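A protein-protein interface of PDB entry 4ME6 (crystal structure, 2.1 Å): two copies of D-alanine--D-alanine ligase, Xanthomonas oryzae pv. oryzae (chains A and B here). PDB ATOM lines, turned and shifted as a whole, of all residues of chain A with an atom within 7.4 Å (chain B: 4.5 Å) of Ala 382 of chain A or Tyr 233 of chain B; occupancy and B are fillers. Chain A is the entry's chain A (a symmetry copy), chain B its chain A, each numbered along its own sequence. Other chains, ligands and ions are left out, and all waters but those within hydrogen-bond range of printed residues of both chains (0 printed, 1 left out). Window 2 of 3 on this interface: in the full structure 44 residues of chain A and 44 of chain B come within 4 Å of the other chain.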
ATOM      1  N   ASP A 376      -7.086 -15.727   2.734  1.00  0.00           N
ATOM      2  CA  ASP A 376      -5.924 -16.018   1.934  1.00  0.00           C
ATOM      3  C   ASP A 376      -6.049 -17.409   1.332  1.00  0.00           C
ATOM      4  O   ASP A 376      -5.517 -17.703   0.246  1.00  0.00           O
ATOM      5  CB  ASP A 376      -4.690 -16.006   2.808  1.00  0.00           C
ATOM      6  CG  ASP A 376      -3.507 -15.395   2.113  1.00  0.00           C
ATOM      7  OD1 ASP A 376      -3.598 -14.166   1.884  1.00  0.00           O
ATOM      8  OD2 ASP A 376      -2.521 -16.114   1.777  1.00  0.00           O
ATOM      9  N   GLN A 377      -6.762 -18.253   2.074  1.00  0.00           N
ATOM     10  CA  GLN A 377      -6.847 -19.673   1.828  1.00  0.00           C
ATOM     11  C   GLN A 377      -7.482 -19.901   0.510  1.00  0.00           C
ATOM     12  O   GLN A 377      -7.000 -20.722  -0.261  1.00  0.00           O
ATOM     13  CB  GLN A 377      -7.709 -20.354   2.890  1.00  0.00           C
ATOM     14  CG  GLN A 377      -7.272 -21.757   3.199  1.00  0.00           C
ATOM     15  CD  GLN A 377      -5.921 -21.799   3.901  1.00  0.00           C
ATOM     16  OE1 GLN A 377      -5.297 -20.764   4.195  1.00  0.00           O
ATOM     17  NE2 GLN A 377      -5.456 -23.010   4.167  1.00  0.00           N
ATOM     18  N   LEU A 378      -8.570 -19.179   0.267  1.00  0.00           N
ATOM     19  CA  LEU A 378      -9.299 -19.305  -0.982  1.00  0.00           C
ATOM     20  C   LEU A 378      -8.465 -18.804  -2.191  1.00  0.00           C
ATOM     21  O   LEU A 378      -8.421 -19.456  -3.243  1.00  0.00           O
ATOM     22  CB  LEU A 378     -10.629 -18.567  -0.885  1.00  0.00           C
ATOM     23  CG  LEU A 378     -11.742 -19.265  -0.081  1.00  0.00           C
ATOM     24  CD1 LEU A 378     -11.313 -19.722   1.309  1.00  0.00           C
ATOM     25  CD2 LEU A 378     -12.946 -18.326   0.018  1.00  0.00           C
ATOM     26  N   LEU A 379      -7.777 -17.675  -2.015  1.00  0.00           N
ATOM     27  CA  LEU A 379      -6.935 -17.082  -3.079  1.00  0.00           C
ATOM     28  C   LEU A 379      -5.702 -17.928  -3.390  1.00  0.00           C
ATOM     29  O   LEU A 379      -5.334 -18.059  -4.555  1.00  0.00           O
ATOM     30  CB  LEU A 379      -6.474 -15.675  -2.715  1.00  0.00           C
ATOM     31  CG  LEU A 379      -7.487 -14.637  -2.205  1.00  0.00           C
ATOM     32  CD1 LEU A 379      -6.699 -13.357  -1.973  1.00  0.00           C
ATOM     33  CD2 LEU A 379      -8.687 -14.371  -3.118  1.00  0.00           C
ATOM     34  N   ARG A 380      -5.071 -18.505  -2.364  1.00  0.00           N
ATOM     35  CA  ARG A 380      -3.917 -19.392  -2.575  1.00  0.00           C
ATOM     36  C   ARG A 380      -4.330 -20.580  -3.430  1.00  0.00           C
ATOM     37  O   ARG A 380      -3.663 -20.917  -4.409  1.00  0.00           O
ATOM     38  CB  ARG A 380      -3.365 -19.916  -1.250  1.00  0.00           C
ATOM     39  CG  ARG A 380      -2.057 -20.691  -1.413  1.00  0.00           C
ATOM     40  CD  ARG A 380      -0.821 -19.850  -1.065  1.00  0.00           C
ATOM     41  NE  ARG A 380      -0.912 -19.330   0.307  1.00  0.00           N
ATOM     42  CZ  ARG A 380      -0.607 -20.001   1.426  1.00  0.00           C
ATOM     43  NH1 ARG A 380      -0.150 -21.243   1.401  1.00  0.00           N
ATOM     44  NH2 ARG A 380      -0.768 -19.416   2.604  1.00  0.00           N
ATOM     45  N   SER A 381      -5.451 -21.183  -3.032  1.00  0.00           N
ATOM     46  CA  SER A 381      -6.059 -22.337  -3.694  1.00  0.00           C
ATOM     47  C   SER A 381      -6.619 -22.079  -5.117  1.00  0.00           C
ATOM     48  O   SER A 381      -7.031 -23.017  -5.778  1.00  0.00           O
ATOM     49  CB  SER A 381      -7.199 -22.868  -2.790  1.00  0.00           C
ATOM     50  OG  SER A 381      -8.191 -21.863  -2.545  1.00  0.00           O
ATOM     51  N   ALA A 382      -6.668 -20.818  -5.558  1.00  0.00           N
ATOM     52  CA  ALA A 382      -7.115 -20.458  -6.919  1.00  0.00           C
ATOM     53  C   ALA A 382      -6.065 -20.722  -8.015  1.00  0.00           C
ATOM     54  O   ALA A 382      -6.403 -20.755  -9.195  1.00  0.00           O
ATOM     55  CB  ALA A 382      -7.570 -19.003  -6.959  1.00  0.00           C
ATOM     56  N   VAL A 383      -4.803 -20.913  -7.640  1.00  0.00           N
ATOM     57  CA  VAL A 383      -3.728 -21.201  -8.621  1.00  0.00           C
ATOM     58  C   VAL A 383      -3.924 -22.529  -9.428  1.00  0.00           C
ATOM     59  O   VAL A 383      -4.374 -23.555  -8.890  1.00  0.00           O
ATOM     60  CB  VAL A 383      -2.329 -21.178  -7.920  1.00  0.00           C
ATOM     61  CG1 VAL A 383      -2.148 -22.367  -6.970  1.00  0.00           C
ATOM     62  CG2 VAL A 383      -1.196 -21.123  -8.938  1.00  0.00           C
ATOM     63  N   GLU A 384      -3.558 -22.514 -10.710  1.00  0.00           N
ATOM     64  CA  GLU A 384      -3.697 -23.701 -11.557  1.00  0.00           C
ATOM     65  C   GLU A 384      -2.444 -24.561 -11.538  1.00  0.00           C
ATOM     66  O   GLU A 384      -2.539 -25.776 -11.641  1.00  0.00           O
ATOM     67  CB  GLU A 384      -4.032 -23.294 -12.991  1.00  0.00           C
ATOM     68  CG  GLU A 384      -5.464 -22.819 -13.165  1.00  0.00           C
ATOM     69  CD  GLU A 384      -5.959 -22.936 -14.594  1.00  0.00           C
ATOM     70  OE1 GLU A 384      -5.164 -22.664 -15.515  1.00  0.00           O
ATOM     71  OE2 GLU A 384      -7.142 -23.300 -14.798  1.00  0.00           O
ATOM     72  N   PRO B 205      -4.647  -8.680 -11.212  1.00  0.00           N
ATOM     73  CA  PRO B 205      -4.544  -8.877  -9.789  1.00  0.00           C
ATOM     74  C   PRO B 205      -3.139  -8.340  -9.376  1.00  0.00           C
ATOM     75  O   PRO B 205      -2.215  -8.439 -10.160  1.00  0.00           O
ATOM     76  CB  PRO B 205      -4.654 -10.398  -9.634  1.00  0.00           C
ATOM     77  CG  PRO B 205      -4.920 -10.953 -11.024  1.00  0.00           C
ATOM     78  CD  PRO B 205      -4.360  -9.912 -11.963  1.00  0.00           C
ATOM     79  N   VAL B 212      -2.176 -14.569 -14.926  1.00  0.00           N
ATOM     80  CA  VAL B 212      -3.519 -15.152 -14.711  1.00  0.00           C
ATOM     81  C   VAL B 212      -4.470 -14.167 -14.015  1.00  0.00           C
ATOM     82  O   VAL B 212      -4.054 -13.423 -13.122  1.00  0.00           O
ATOM     83  CB  VAL B 212      -3.474 -16.480 -13.885  1.00  0.00           C
ATOM     84  CG1 VAL B 212      -3.290 -16.228 -12.380  1.00  0.00           C
ATOM     85  CG2 VAL B 212      -4.736 -17.299 -14.138  1.00  0.00           C
ATOM     86  N   GLY B 213      -5.747 -14.178 -14.402  1.00  0.00           N
ATOM     87  CA  GLY B 213      -6.706 -13.170 -13.926  1.00  0.00           C
ATOM     88  C   GLY B 213      -6.551 -11.809 -14.621  1.00  0.00           C
ATOM     89  O   GLY B 213      -7.229 -10.829 -14.275  1.00  0.00           O
ATOM     90  N   LEU B 229     -13.264 -11.465 -12.131  1.00  0.00           N
ATOM     91  CA  LEU B 229     -12.284 -12.554 -12.332  1.00  0.00           C
ATOM     92  C   LEU B 229     -10.972 -12.341 -11.544  1.00  0.00           C
ATOM     93  O   LEU B 229     -10.448 -13.232 -10.874  1.00  0.00           O
ATOM     94  CB  LEU B 229     -11.937 -12.621 -13.819  1.00  0.00           C
ATOM     95  CG  LEU B 229     -11.534 -13.906 -14.543  1.00  0.00           C
ATOM     96  CD1 LEU B 229     -10.559 -13.576 -15.658  1.00  0.00           C
ATOM     97  CD2 LEU B 229     -10.930 -14.963 -13.627  1.00  0.00           C
ATOM     98  N   ALA B 230     -10.425 -11.146 -11.649  1.00  0.00           N
ATOM     99  CA  ALA B 230      -9.183 -10.812 -10.976  1.00  0.00           C
ATOM    100  C   ALA B 230      -9.301 -10.951  -9.458  1.00  0.00           C
ATOM    101  O   ALA B 230      -8.392 -11.430  -8.762  1.00  0.00           O
ATOM    102  CB  ALA B 230      -8.793  -9.398 -11.308  1.00  0.00           C
ATOM    103  N   LEU B 231     -10.417 -10.493  -8.936  1.00  0.00           N
ATOM    104  CA  LEU B 231     -10.615 -10.564  -7.526  1.00  0.00           C
ATOM    105  C   LEU B 231     -10.727 -12.001  -7.007  1.00  0.00           C
ATOM    106  O   LEU B 231     -10.628 -12.201  -5.822  1.00  0.00           O
ATOM    107  CB  LEU B 231     -11.841  -9.735  -7.133  1.00  0.00           C
ATOM    108  CG  LEU B 231     -11.637  -8.238  -6.998  1.00  0.00           C
ATOM    109  CD1 LEU B 231     -12.979  -7.533  -6.924  1.00  0.00           C
ATOM    110  CD2 LEU B 231     -10.841  -7.903  -5.742  1.00  0.00           C
ATOM    111  N   ALA B 232     -10.908 -12.994  -7.865  1.00  0.00           N
ATOM    112  CA  ALA B 232     -10.815 -14.399  -7.418  1.00  0.00           C
ATOM    113  C   ALA B 232      -9.403 -14.832  -7.113  1.00  0.00           C
ATOM    114  O   ALA B 232      -9.186 -15.814  -6.450  1.00  0.00           O
ATOM    115  CB  ALA B 232     -11.409 -15.324  -8.448  1.00  0.00           C
ATOM    116  N   TYR B 233      -8.424 -14.098  -7.613  1.00  0.00           N
ATOM    117  CA  TYR B 233      -7.028 -14.447  -7.425  1.00  0.00           C
ATOM    118  C   TYR B 233      -6.339 -13.617  -6.367  1.00  0.00           C
ATOM    119  O   TYR B 233      -5.547 -14.148  -5.632  1.00  0.00           O
ATOM    120  CB  TYR B 233      -6.279 -14.291  -8.739  1.00  0.00           C
ATOM    121  CG  TYR B 233      -6.634 -15.360  -9.716  1.00  0.00           C
ATOM    122  CD1 TYR B 233      -7.663 -15.187 -10.644  1.00  0.00           C
ATOM    123  CD2 TYR B 233      -5.931 -16.549  -9.716  1.00  0.00           C
ATOM    124  CE1 TYR B 233      -7.976 -16.180 -11.547  1.00  0.00           C
ATOM    125  CE2 TYR B 233      -6.233 -17.553 -10.596  1.00  0.00           C
ATOM    126  CZ  TYR B 233      -7.253 -17.375 -11.514  1.00  0.00           C
ATOM    127  OH  TYR B 233      -7.524 -18.420 -12.377  1.00  0.00           O
ATOM    128  N   ASP B 234      -6.623 -12.324  -6.277  1.00  0.00           N
ATOM    129  CA  ASP B 234      -6.006 -11.505  -5.250  1.00  0.00           C
ATOM    130  C   ASP B 234      -7.059 -10.676  -4.560  1.00  0.00           C
ATOM    131  O   ASP B 234      -8.172 -10.463  -5.081  1.00  0.00           O
ATOM    132  CB  ASP B 234      -4.864 -10.602  -5.815  1.00  0.00           C
ATOM    133  CG  ASP B 234      -3.781 -10.292  -4.760  1.00  0.00           C
ATOM    134  OD1 ASP B 234      -3.659 -11.158  -3.861  1.00  0.00           O
ATOM    135  OD2 ASP B 234      -3.044  -9.237  -4.789  1.00  0.00           O
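Of the 9 printed residues of chain B, 4 touch a printed residue of chain A. Printed residues of chain B that touch a printed residue of chain A: Leu 231, Ala 232, Tyr 233 and Asp 234. Hydrophobic or aromatic side chains of chain B within 4 Å of the printed part of chain A: Tyr 233. Of the 9 printed residues of chain A, 2 touch a printed residue of chain B. Among the printed residues, no Asp or Glu carboxylate lies within 4 Å of a Lys or Arg side-chain nitrogen of the other chain.
No position is printed for both chains.
Of the printed residues of chain B, Leu 379 of chain A touches Leu 231, Ala 232, Tyr 233 and Asp 234. Of chain B, only Ala 232 and Tyr 233 come within 4 Å of Ala 382 of chain A. Printed residues of chain A within 4 Å of Leu 231 of chain B: Leu 379 (3.97 Å). Of chain A, only Leu 379 and Ala 382 come within 4 Å of Ala 232 of chain B. Printed residues of chain A within 4 Å of Tyr 233 of chain B: Leu 379 (3.4 Å) and Ala 382 (3.5 Å). Of the printed residues of chain A, Asp 234 of chain B touches Leu 379 (3.7 Å). The nearest printed residue of chain B that does not touch Ala 382 of chain A is Val 212 of chain B (6.3 Å). The nearest residue of chain A that does not touch Tyr 233 of chain B is Val 383 of chain A (4.7 Å).
Among the printed residues, pairs that only touch across the chains: Leu 379 of chain A with Tyr 233 of chain B (3.4 Å), Ala 382 of chain A with Tyr 233 of chain B (3.5 Å), Ala 382 of chain A with Ala 232 of chain B (3.6 Å), Leu 379 of chain A with Ala 232 of chain B (3.7 Å), Leu 379 of chain A with Asp 234 of chain B (3.7 Å) and Leu 379 of chain A with Leu 231 of chain B (3.97 Å).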
